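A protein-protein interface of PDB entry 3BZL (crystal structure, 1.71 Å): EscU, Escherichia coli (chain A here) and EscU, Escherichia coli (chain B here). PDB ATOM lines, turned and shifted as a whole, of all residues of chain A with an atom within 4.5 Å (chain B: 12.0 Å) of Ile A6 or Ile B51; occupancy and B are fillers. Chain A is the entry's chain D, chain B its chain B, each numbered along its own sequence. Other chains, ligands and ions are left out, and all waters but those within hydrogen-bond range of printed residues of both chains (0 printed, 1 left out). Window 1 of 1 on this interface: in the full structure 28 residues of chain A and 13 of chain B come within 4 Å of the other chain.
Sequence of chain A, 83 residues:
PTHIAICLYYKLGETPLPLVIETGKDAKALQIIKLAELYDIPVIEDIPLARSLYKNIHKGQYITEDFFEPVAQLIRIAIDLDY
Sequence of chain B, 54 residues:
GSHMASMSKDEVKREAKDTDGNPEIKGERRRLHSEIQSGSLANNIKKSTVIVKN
Val B52 touches Ala A5.
O of Val B50 touches O of Ile A6, at 3.9 Å.
Val B52 touches Leu A8 (CG2 to CD1, 3.8 Å).
Leu B41 touches Glu A22 (CA to OE2, 3.7 Å).
CD1 of Ile B45 touches CG2 of Ile A32, 3.9 Å away.
CG2 of Ile A41 touches OG of Ser B48, at 3.4 Å.
Ile A41 touches Val B50 (CG2 to N, 3.97 Å).
O of Pro A42 touches CA of Val B50, 3.5 Å away.
Val A43 touches Ile B51 (CA to O, 3.4 Å).
Lys B53 touches Ala A50.
Ala A5 touches just one residue of chain B: Val B52.
Leu A8 touches four residues of chain B.
No residue of chain B comes within 4 Å of Val A20.
Of chain B, only Ile B45 (3.7 Å) and Ile B51 (3.9 Å) come within 4 Å of Ala A36.
Of chain B, only Thr B49, Val B50 and Ile B51 come within 4 Å of Pro A42.
Val A43 touches just these residues of chain B: Ile B51 and Lys B53.
Ile A44 touches just these residues of chain B: Ile B51 (2.9 Å), Val B52 (3.3 Å) and Lys B53 (3.0 Å).
Of chain B, only Val B52, Lys B53 and Asn B54 come within 4 Å of Ala A50.
Tyr A54 touches none of the printed residues of chain B.
Of the printed residues of chain A, Ile B45 touches Cys A7, Ile A32, Ala A36 and Ile A41.
Printed residues of chain A within 4 Å of Ile B51: Ile A6 (3.3 Å), Ala A36 (3.9 Å), Ile A41 (3.4 Å), Pro A42 (2.9 Å), Val A43 (3.4 Å) and Ile A44 (2.9 Å).
Of the printed residues of chain A, Lys B53 touches Ile A4, Val A43, Ile A44 and Ala A50.
The nearest residue of chain B that does not touch Ile A6 is Lys B53 (5.0 Å).
Of the 17 printed residues of chain A, 13 touch a printed residue of chain B.
Printed residues of chain A that touch a printed residue of chain B: Ile A4, Ala A5, Ile A6, Cys A7, Leu A8, Glu A22, Ile A32, Ala A36, Ile A41, Pro A42, Val A43, Ile A44 and Ala A50.
Among the printed residues, 35 pairs touch across the chains.
ND2 of Asn B44 sits close to O of Ser B40 (3.5 Å).
O of Ile B45 sits at hydrogen-bond distance from OG of Ser B48.
O of Glu A22 lies within hydrogen-bond range of N of Cys A7.
The backbone carbonyl oxygen (O) of Ala A36 sits at hydrogen-bond distance from the backbone NH (N) of Ile A41 (2.9 Å).
The side-chain amide oxygen (OD1) of Asn B54 lies within hydrogen-bond range of the backbone NH (N) of Ile A4 (2.9 Å).
The backbone NH (N) of Ile A6 is in hydrogen-bond range of the backbone carbonyl oxygen (O) of Val B52, 2.8 Å away.
The backbone carbonyl oxygen (O) of Val B50 is in hydrogen-bond range of the backbone NH (N) of Leu A8, 2.9 Å away.
The backbone carbonyl oxygen of Leu A8 lies within hydrogen-bond range of the backbone NH of Thr B49 (2.8 Å).
The backbone NH (N) of Lys B53 sits at hydrogen-bond distance from the backbone carbonyl oxygen (O) of Ile A44, 3.0 Å away.
OG of Ser B48 sits close to SG of Cys A7 (3.3 Å).
The backbone NH of Ile A44 lies within hydrogen-bond range of the backbone carbonyl oxygen of Ile B51, at 2.9 Å.
The backbone NH of Ile B51 sits at hydrogen-bond distance from the backbone carbonyl oxygen of Pro A42.
ND2 of Asn B44 is in hydrogen-bond range of OE2 of Glu A22, 2.4 Å away.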
ATOM      1  N   ILE A   4      -2.335  10.814  10.247  1.00  0.00           N
ATOM      2  CA  ILE A   4      -3.605  10.287  10.739  1.00  0.00           C
ATOM      3  C   ILE A   4      -4.575  11.457  10.934  1.00  0.00           C
ATOM      4  O   ILE A   4      -4.185  12.518  11.443  1.00  0.00           O
ATOM      5  CB  ILE A   4      -3.416   9.616  12.104  1.00  0.00           C
ATOM      6  CG1 ILE A   4      -2.474   8.417  12.012  1.00  0.00           C
ATOM      7  CG2 ILE A   4      -4.757   9.186  12.709  1.00  0.00           C
ATOM      8  CD1 ILE A   4      -2.236   7.806  13.378  1.00  0.00           C
ATOM      9  N   ALA A   5      -5.835  11.263  10.554  1.00  0.00           N
ATOM     10  CA  ALA A   5      -6.887  12.242  10.846  1.00  0.00           C
ATOM     11  C   ALA A   5      -8.137  11.466  11.216  1.00  0.00           C
ATOM     12  O   ALA A   5      -8.458  10.448  10.593  1.00  0.00           O
ATOM     13  CB  ALA A   5      -7.146  13.147   9.658  1.00  0.00           C
ATOM     14  N   ILE A   6      -8.768  11.916  12.281  1.00  0.00           N
ATOM     15  CA  ILE A   6     -10.009  11.333  12.775  1.00  0.00           C
ATOM     16  C   ILE A   6     -11.082  12.412  12.792  1.00  0.00           C
ATOM     17  O   ILE A   6     -10.899  13.442  13.424  1.00  0.00           O
ATOM     18  CB  ILE A   6      -9.863  10.806  14.230  1.00  0.00           C
ATOM     19  CG1 ILE A   6      -8.632   9.928  14.427  1.00  0.00           C
ATOM     20  CG2 ILE A   6     -11.154  10.072  14.675  1.00  0.00           C
ATOM     21  CD1 ILE A   6      -8.632   8.659  13.635  1.00  0.00           C
ATOM     22  N   CYS A   7     -12.193  12.203  12.094  1.00  0.00           N
ATOM     23  CA  CYS A   7     -13.297  13.139  12.064  1.00  0.00           C
ATOM     24  C   CYS A   7     -14.327  12.725  13.112  1.00  0.00           C
ATOM     25  O   CYS A   7     -14.869  11.631  13.021  1.00  0.00           O
ATOM     26  CB  CYS A   7     -13.915  13.114  10.658  1.00  0.00           C
ATOM     27  SG  CYS A   7     -15.241  14.301  10.317  1.00  0.00           S
ATOM     28  N   LEU A   8     -14.583  13.604  14.061  1.00  0.00           N
ATOM     29  CA  LEU A   8     -15.555  13.355  15.126  1.00  0.00           C
ATOM     30  C   LEU A   8     -16.814  14.181  14.922  1.00  0.00           C
ATOM     31  O   LEU A   8     -16.761  15.384  14.594  1.00  0.00           O
ATOM     32  CB  LEU A   8     -14.941  13.669  16.476  1.00  0.00           C
ATOM     33  CG  LEU A   8     -13.843  12.714  16.941  1.00  0.00           C
ATOM     34  CD1 LEU A   8     -13.046  13.434  18.007  1.00  0.00           C
ATOM     35  CD2 LEU A   8     -14.463  11.439  17.493  1.00  0.00           C
ATOM     36  N   VAL A  20     -17.075   8.517  15.438  1.00  0.00           N
ATOM     37  CA  VAL A  20     -15.998   8.628  14.452  1.00  0.00           C
ATOM     38  C   VAL A  20     -16.651   8.414  13.104  1.00  0.00           C
ATOM     39  O   VAL A  20     -17.005   7.301  12.749  1.00  0.00           O
ATOM     40  CB  VAL A  20     -14.898   7.623  14.718  1.00  0.00           C
ATOM     41  CG1 VAL A  20     -13.930   7.616  13.580  1.00  0.00           C
ATOM     42  CG2 VAL A  20     -14.199   8.008  16.037  1.00  0.00           C
ATOM     43  N   GLU A  22     -15.408   9.535  10.008  1.00  0.00           N
ATOM     44  CA  GLU A  22     -14.417   9.314   8.971  1.00  0.00           C
ATOM     45  C   GLU A  22     -13.066   9.207   9.637  1.00  0.00           C
ATOM     46  O   GLU A  22     -12.826   9.834  10.664  1.00  0.00           O
ATOM     47  CB  GLU A  22     -14.374  10.473   7.982  1.00  0.00           C
ATOM     48  CG  GLU A  22     -15.553  10.593   7.073  1.00  0.00           C
ATOM     49  CD  GLU A  22     -15.520   9.593   5.908  1.00  0.00           C
ATOM     50  OE1 GLU A  22     -14.498   8.901   5.686  1.00  0.00           O
ATOM     51  OE2 GLU A  22     -16.539   9.513   5.204  1.00  0.00           O
ATOM     52  N   THR A  23     -12.193   8.411   9.031  1.00  0.00           N
ATOM     53  CA  THR A  23     -10.842   8.236   9.516  1.00  0.00           C
ATOM     54  C   THR A  23      -9.975   8.117   8.270  1.00  0.00           C
ATOM     55  O   THR A  23     -10.468   7.712   7.197  1.00  0.00           O
ATOM     56  CB  THR A  23     -10.751   6.984  10.436  1.00  0.00           C
ATOM     57  OG1 THR A  23      -9.409   6.785  10.909  1.00  0.00           O
ATOM     58  CG2 THR A  23     -11.206   5.749   9.696  1.00  0.00           C
ATOM     59  N   ILE A  32      -8.719  14.733   4.451  1.00  0.00           N
ATOM     60  CA  ILE A  32      -9.670  15.051   5.524  1.00  0.00           C
ATOM     61  C   ILE A  32      -9.327  16.438   6.076  1.00  0.00           C
ATOM     62  O   ILE A  32     -10.206  17.264   6.288  1.00  0.00           O
ATOM     63  CB  ILE A  32      -9.659  13.954   6.658  1.00  0.00           C
ATOM     64  CG1 ILE A  32     -10.314  12.646   6.172  1.00  0.00           C
ATOM     65  CG2 ILE A  32     -10.359  14.438   7.962  1.00  0.00           C
ATOM     66  CD1 ILE A  32      -9.971  11.388   7.037  1.00  0.00           C
ATOM     67  N   ALA A  36     -11.539  19.710   5.908  1.00  0.00           N
ATOM     68  CA  ALA A  36     -11.892  20.348   7.190  1.00  0.00           C
ATOM     69  C   ALA A  36     -11.636  21.848   7.112  1.00  0.00           C
ATOM     70  O   ALA A  36     -12.452  22.674   7.527  1.00  0.00           O
ATOM     71  CB  ALA A  36     -11.080  19.714   8.334  1.00  0.00           C
ATOM     72  N   ILE A  41     -14.053  23.501   9.771  1.00  0.00           N
ATOM     73  CA  ILE A  41     -14.196  22.582  10.896  1.00  0.00           C
ATOM     74  C   ILE A  41     -12.891  22.722  11.687  1.00  0.00           C
ATOM     75  O   ILE A  41     -11.802  22.671  11.103  1.00  0.00           O
ATOM     76  CB  ILE A  41     -14.338  21.101  10.446  1.00  0.00           C
ATOM     77  CG1 ILE A  41     -15.363  20.946   9.331  1.00  0.00           C
ATOM     78  CG2 ILE A  41     -14.693  20.223  11.650  1.00  0.00           C
ATOM     79  CD1 ILE A  41     -16.709  21.248   9.754  1.00  0.00           C
ATOM     80  N   PRO A  42     -12.985  22.908  13.002  1.00  0.00           N
ATOM     81  CA  PRO A  42     -11.725  22.997  13.762  1.00  0.00           C
ATOM     82  C   PRO A  42     -10.908  21.737  13.653  1.00  0.00           C
ATOM     83  O   PRO A  42     -11.448  20.632  13.736  1.00  0.00           O
ATOM     84  CB  PRO A  42     -12.175  23.201  15.199  1.00  0.00           C
ATOM     85  CG  PRO A  42     -13.628  23.333  15.165  1.00  0.00           C
ATOM     86  CD  PRO A  42     -14.167  22.980  13.880  1.00  0.00           C
ATOM     87  N   VAL A  43      -9.594  21.921  13.506  1.00  0.00           N
ATOM     88  CA  VAL A  43      -8.637  20.851  13.451  1.00  0.00           C
ATOM     89  C   VAL A  43      -7.669  21.038  14.603  1.00  0.00           C
ATOM     90  O   VAL A  43      -7.096  22.122  14.762  1.00  0.00           O
ATOM     91  CB  VAL A  43      -7.844  20.871  12.123  1.00  0.00           C
ATOM     92  CG1 VAL A  43      -6.760  19.783  12.131  1.00  0.00           C
ATOM     93  CG2 VAL A  43      -8.814  20.737  10.916  1.00  0.00           C
ATOM     94  N   ILE A  44      -7.486  19.983  15.396  1.00  0.00           N
ATOM     95  CA  ILE A  44      -6.605  20.014  16.549  1.00  0.00           C
ATOM     96  C   ILE A  44      -5.596  18.884  16.456  1.00  0.00           C
ATOM     97  O   ILE A  44      -5.954  17.727  16.265  1.00  0.00           O
ATOM     98  CB  ILE A  44      -7.392  19.809  17.864  1.00  0.00           C
ATOM     99  CG1 ILE A  44      -8.507  20.821  17.976  1.00  0.00           C
ATOM    100  CG2 ILE A  44      -6.411  19.903  19.051  1.00  0.00           C
ATOM    101  CD1 ILE A  44      -8.039  22.193  18.091  1.00  0.00           C
ATOM    102  N   ALA A  50      -4.900  11.021  18.568  1.00  0.00           N
ATOM    103  CA  ALA A  50      -5.108  10.614  17.181  1.00  0.00           C
ATOM    104  C   ALA A  50      -4.682   9.160  16.983  1.00  0.00           C
ATOM    105  O   ALA A  50      -5.422   8.374  16.396  1.00  0.00           O
ATOM    106  CB  ALA A  50      -4.334  11.523  16.245  1.00  0.00           C
ATOM    107  N   LEU A  53      -7.177   6.722  18.891  1.00  0.00           N
ATOM    108  CA  LEU A  53      -8.463   6.658  18.194  1.00  0.00           C
ATOM    109  C   LEU A  53      -8.340   5.830  16.914  1.00  0.00           C
ATOM    110  O   LEU A  53      -9.172   4.970  16.621  1.00  0.00           O
ATOM    111  CB  LEU A  53      -8.952   8.076  17.871  1.00  0.00           C
ATOM    112  CG  LEU A  53      -9.537   8.890  19.037  1.00  0.00           C
ATOM    113  CD1 LEU A  53      -9.735  10.345  18.614  1.00  0.00           C
ATOM    114  CD2 LEU A  53     -10.832   8.301  19.481  1.00  0.00           C
ATOM    115  N   TYR A  54      -7.285   6.065  16.156  1.00  0.00           N
ATOM    116  CA  TYR A  54      -7.104   5.367  14.891  1.00  0.00           C
ATOM    117  C   TYR A  54      -7.050   3.867  15.101  1.00  0.00           C
ATOM    118  O   TYR A  54      -7.629   3.097  14.335  1.00  0.00           O
ATOM    119  CB  TYR A  54      -5.846   5.860  14.201  1.00  0.00           C
ATOM    120  CG  TYR A  54      -5.694   5.291  12.826  1.00  0.00           C
ATOM    121  CD1 TYR A  54      -6.487   5.743  11.771  1.00  0.00           C
ATOM    122  CD2 TYR A  54      -4.784   4.277  12.579  1.00  0.00           C
ATOM    123  CE1 TYR A  54      -6.356   5.216  10.517  1.00  0.00           C
ATOM    124  CE2 TYR A  54      -4.645   3.745  11.329  1.00  0.00           C
ATOM    125  CZ  TYR A  54      -5.431   4.211  10.296  1.00  0.00           C
ATOM    126  OH  TYR A  54      -5.279   3.662   9.049  1.00  0.00           O
ATOM    127  N   SER B  40     -20.791  10.240   1.690  1.00  0.00           N
ATOM    128  CA  SER B  40     -19.621  10.742   0.994  1.00  0.00           C
ATOM    129  C   SER B  40     -18.690  11.383   2.004  1.00  0.00           C
ATOM    130  O   SER B  40     -19.134  11.876   3.048  1.00  0.00           O
ATOM    131  CB  SER B  40     -20.020  11.758  -0.078  1.00  0.00           C
ATOM    132  OG  SER B  40     -20.449  12.979   0.494  1.00  0.00           O
ATOM    133  N   LEU B  41     -17.403  11.374   1.678  1.00  0.00           N
ATOM    134  CA  LEU B  41     -16.392  12.009   2.505  1.00  0.00           C
ATOM    135  C   LEU B  41     -16.790  13.470   2.711  1.00  0.00           C
ATOM    136  O   LEU B  41     -16.786  13.982   3.829  1.00  0.00           O
ATOM    137  CB  LEU B  41     -15.049  11.951   1.775  1.00  0.00           C
ATOM    138  CG  LEU B  41     -13.703  11.798   2.484  1.00  0.00           C
ATOM    139  CD1 LEU B  41     -12.605  12.502   1.657  1.00  0.00           C
ATOM    140  CD2 LEU B  41     -13.704  12.261   3.896  1.00  0.00           C
ATOM    141  N   ALA B  42     -17.150  14.146   1.623  1.00  0.00           N
ATOM    142  CA  ALA B  42     -17.433  15.571   1.715  1.00  0.00           C
ATOM    143  C   ALA B  42     -18.599  15.825   2.665  1.00  0.00           C
ATOM    144  O   ALA B  42     -18.503  16.692   3.524  1.00  0.00           O
ATOM    145  CB  ALA B  42     -17.729  16.153   0.343  1.00  0.00           C
ATOM    146  N   ASN B  43     -19.686  15.071   2.521  1.00  0.00           N
ATOM    147  CA  ASN B  43     -20.869  15.246   3.382  1.00  0.00           C
ATOM    148  C   ASN B  43     -20.507  15.025   4.851  1.00  0.00           C
ATOM    149  O   ASN B  43     -20.953  15.776   5.735  1.00  0.00           O
ATOM    150  CB  ASN B  43     -21.967  14.286   2.942  1.00  0.00           C
ATOM    151  CG  ASN B  43     -23.245  14.417   3.760  1.00  0.00           C
ATOM    152  OD1 ASN B  43     -24.214  15.051   3.325  1.00  0.00           O
ATOM    153  ND2 ASN B  43     -23.268  13.792   4.930  1.00  0.00           N
ATOM    154  N   ASN B  44     -19.683  14.010   5.101  1.00  0.00           N
ATOM    155  CA  ASN B  44     -19.278  13.670   6.472  1.00  0.00           C
ATOM    156  C   ASN B  44     -18.417  14.771   7.090  1.00  0.00           C
ATOM    157  O   ASN B  44     -18.636  15.170   8.232  1.00  0.00           O
ATOM    158  CB  ASN B  44     -18.512  12.339   6.520  1.00  0.00           C
ATOM    159  CG  ASN B  44     -19.410  11.129   6.296  1.00  0.00           C
ATOM    160  OD1 ASN B  44     -20.635  11.212   6.418  1.00  0.00           O
ATOM    161  ND2 ASN B  44     -18.792   9.987   5.970  1.00  0.00           N
ATOM    162  N   ILE B  45     -17.445  15.279   6.346  1.00  0.00           N
ATOM    163  CA  ILE B  45     -16.599  16.339   6.876  1.00  0.00           C
ATOM    164  C   ILE B  45     -17.415  17.609   7.121  1.00  0.00           C
ATOM    165  O   ILE B  45     -17.305  18.253   8.170  1.00  0.00           O
ATOM    166  CB  ILE B  45     -15.411  16.663   5.964  1.00  0.00           C
ATOM    167  CG1 ILE B  45     -14.567  15.426   5.686  1.00  0.00           C
ATOM    168  CG2 ILE B  45     -14.568  17.767   6.593  1.00  0.00           C
ATOM    169  CD1 ILE B  45     -14.068  14.747   6.892  1.00  0.00           C
ATOM    170  N   LYS B  46     -18.300  17.946   6.186  1.00  0.00           N
ATOM    171  CA  LYS B  46     -19.046  19.202   6.281  1.00  0.00           C
ATOM    172  C   LYS B  46     -19.846  19.300   7.573  1.00  0.00           C
ATOM    173  O   LYS B  46     -19.966  20.380   8.141  1.00  0.00           O
ATOM    174  CB  LYS B  46     -19.988  19.359   5.084  1.00  0.00           C
ATOM    175  CG  LYS B  46     -20.693  20.708   5.041  1.00  0.00           C
ATOM    176  CD  LYS B  46     -21.554  20.854   3.821  1.00  0.00           C
ATOM    177  CE  LYS B  46     -22.248  22.196   3.827  1.00  0.00           C
ATOM    178  NZ  LYS B  46     -23.025  22.345   2.581  1.00  0.00           N
ATOM    179  N   LYS B  47     -20.392  18.179   8.030  1.00  0.00           N
ATOM    180  CA  LYS B  47     -21.251  18.188   9.215  1.00  0.00           C
ATOM    181  C   LYS B  47     -20.493  17.921  10.499  1.00  0.00           C
ATOM    182  O   LYS B  47     -21.084  18.002  11.591  1.00  0.00           O
ATOM    183  CB  LYS B  47     -22.383  17.173   9.082  1.00  0.00           C
ATOM    184  CG  LYS B  47     -21.988  15.732   9.215  1.00  0.00           C
ATOM    185  CD  LYS B  47     -23.223  14.890   8.932  1.00  0.00           C
ATOM    186  CE  LYS B  47     -23.027  13.426   9.147  1.00  0.00           C
ATOM    187  NZ  LYS B  47     -24.369  12.748   9.063  1.00  0.00           N
ATOM    188  N   SER B  48     -19.214  17.640  10.373  1.00  0.00           N
ATOM    189  CA  SER B  48     -18.439  17.179  11.511  1.00  0.00           C
ATOM    190  C   SER B  48     -18.170  18.306  12.506  1.00  0.00           C
ATOM    191  O   SER B  48     -18.382  19.497  12.228  1.00  0.00           O
ATOM    192  CB  SER B  48     -17.150  16.530  11.096  1.00  0.00           C
ATOM    193  OG  SER B  48     -16.331  17.445  10.429  1.00  0.00           O
ATOM    194  N   THR B  49     -17.715  17.883  13.667  1.00  0.00           N
ATOM    195  CA  THR B  49     -17.573  18.749  14.830  1.00  0.00           C
ATOM    196  C   THR B  49     -16.139  19.169  15.048  1.00  0.00           C
ATOM    197  O   THR B  49     -15.864  20.371  15.215  1.00  0.00           O
ATOM    198  CB  THR B  49     -18.120  18.043  16.085  1.00  0.00           C
ATOM    199  OG1 THR B  49     -19.462  17.598  15.800  1.00  0.00           O
ATOM    200  CG2 THR B  49     -18.167  19.025  17.294  1.00  0.00           C
ATOM    201  N   VAL B  50     -15.237  18.195  15.022  1.00  0.00           N
ATOM    202  CA  VAL B  50     -13.811  18.456  15.187  1.00  0.00           C
ATOM    203  C   VAL B  50     -13.001  17.356  14.520  1.00  0.00           C
ATOM    204  O   VAL B  50     -13.457  16.224  14.433  1.00  0.00           O
ATOM    205  CB  VAL B  50     -13.468  18.595  16.690  1.00  0.00           C
ATOM    206  CG1 VAL B  50     -13.725  17.281  17.403  1.00  0.00           C
ATOM    207  CG2 VAL B  50     -12.013  19.094  16.913  1.00  0.00           C
ATOM    208  N   ILE B  51     -11.827  17.722  14.032  1.00  0.00           N
ATOM    209  CA  ILE B  51     -10.901  16.762  13.464  1.00  0.00           C
ATOM    210  C   ILE B  51      -9.716  16.706  14.406  1.00  0.00           C
ATOM    211  O   ILE B  51      -9.172  17.732  14.786  1.00  0.00           O
ATOM    212  CB  ILE B  51     -10.457  17.128  12.023  1.00  0.00           C
ATOM    213  CG1 ILE B  51     -11.542  16.760  10.997  1.00  0.00           C
ATOM    214  CG2 ILE B  51      -9.242  16.332  11.617  1.00  0.00           C
ATOM    215  CD1 ILE B  51     -12.744  17.527  11.046  1.00  0.00           C
ATOM    216  N   VAL B  52      -9.319  15.496  14.758  1.00  0.00           N
ATOM    217  CA  VAL B  52      -8.104  15.260  15.557  1.00  0.00           C
ATOM    218  C   VAL B  52      -7.050  14.661  14.644  1.00  0.00           C
ATOM    219  O   VAL B  52      -7.321  13.674  13.965  1.00  0.00           O
ATOM    220  CB  VAL B  52      -8.372  14.265  16.661  1.00  0.00           C
ATOM    221  CG1 VAL B  52      -7.079  14.076  17.518  1.00  0.00           C
ATOM    222  CG2 VAL B  52      -9.526  14.739  17.537  1.00  0.00           C
ATOM    223  N   LYS B  53      -5.845  15.220  14.645  1.00  0.00           N
ATOM    224  CA  LYS B  53      -4.815  14.748  13.757  1.00  0.00           C
ATOM    225  C   LYS B  53      -3.517  14.538  14.515  1.00  0.00           C
ATOM    226  O   LYS B  53      -3.339  15.030  15.645  1.00  0.00           O
ATOM    227  CB  LYS B  53      -4.618  15.724  12.596  1.00  0.00           C
ATOM    228  CG  LYS B  53      -3.947  17.010  12.989  1.00  0.00           C
ATOM    229  CD  LYS B  53      -3.644  17.858  11.790  1.00  0.00           C
ATOM    230  CE  LYS B  53      -2.815  19.037  12.173  1.00  0.00           C
ATOM    231  NZ  LYS B  53      -1.357  18.645  12.322  1.00  0.00           N
ATOM    232  N   ASN B  54      -2.623  13.766  13.921  1.00  0.00           N
ATOM    233  CA  ASN B  54      -1.295  13.630  14.486  1.00  0.00           C
ATOM    234  C   ASN B  54      -0.351  14.651  13.851  1.00  0.00           C
ATOM    235  O   ASN B  54      -0.796  15.648  13.256  1.00  0.00           O
ATOM    236  CB  ASN B  54      -0.792  12.212  14.263  1.00  0.00           C
ATOM    237  CG  ASN B  54      -0.372  11.955  12.819  1.00  0.00           C
ATOM    238  OD1 ASN B  54      -0.821  12.639  11.876  1.00  0.00           O
ATOM    239  ND2 ASN B  54       0.515  10.969  12.637  1.00  0.00           N
ATOM    240  OXT ASN B  54       0.887  14.506  13.888  1.00  0.00           O
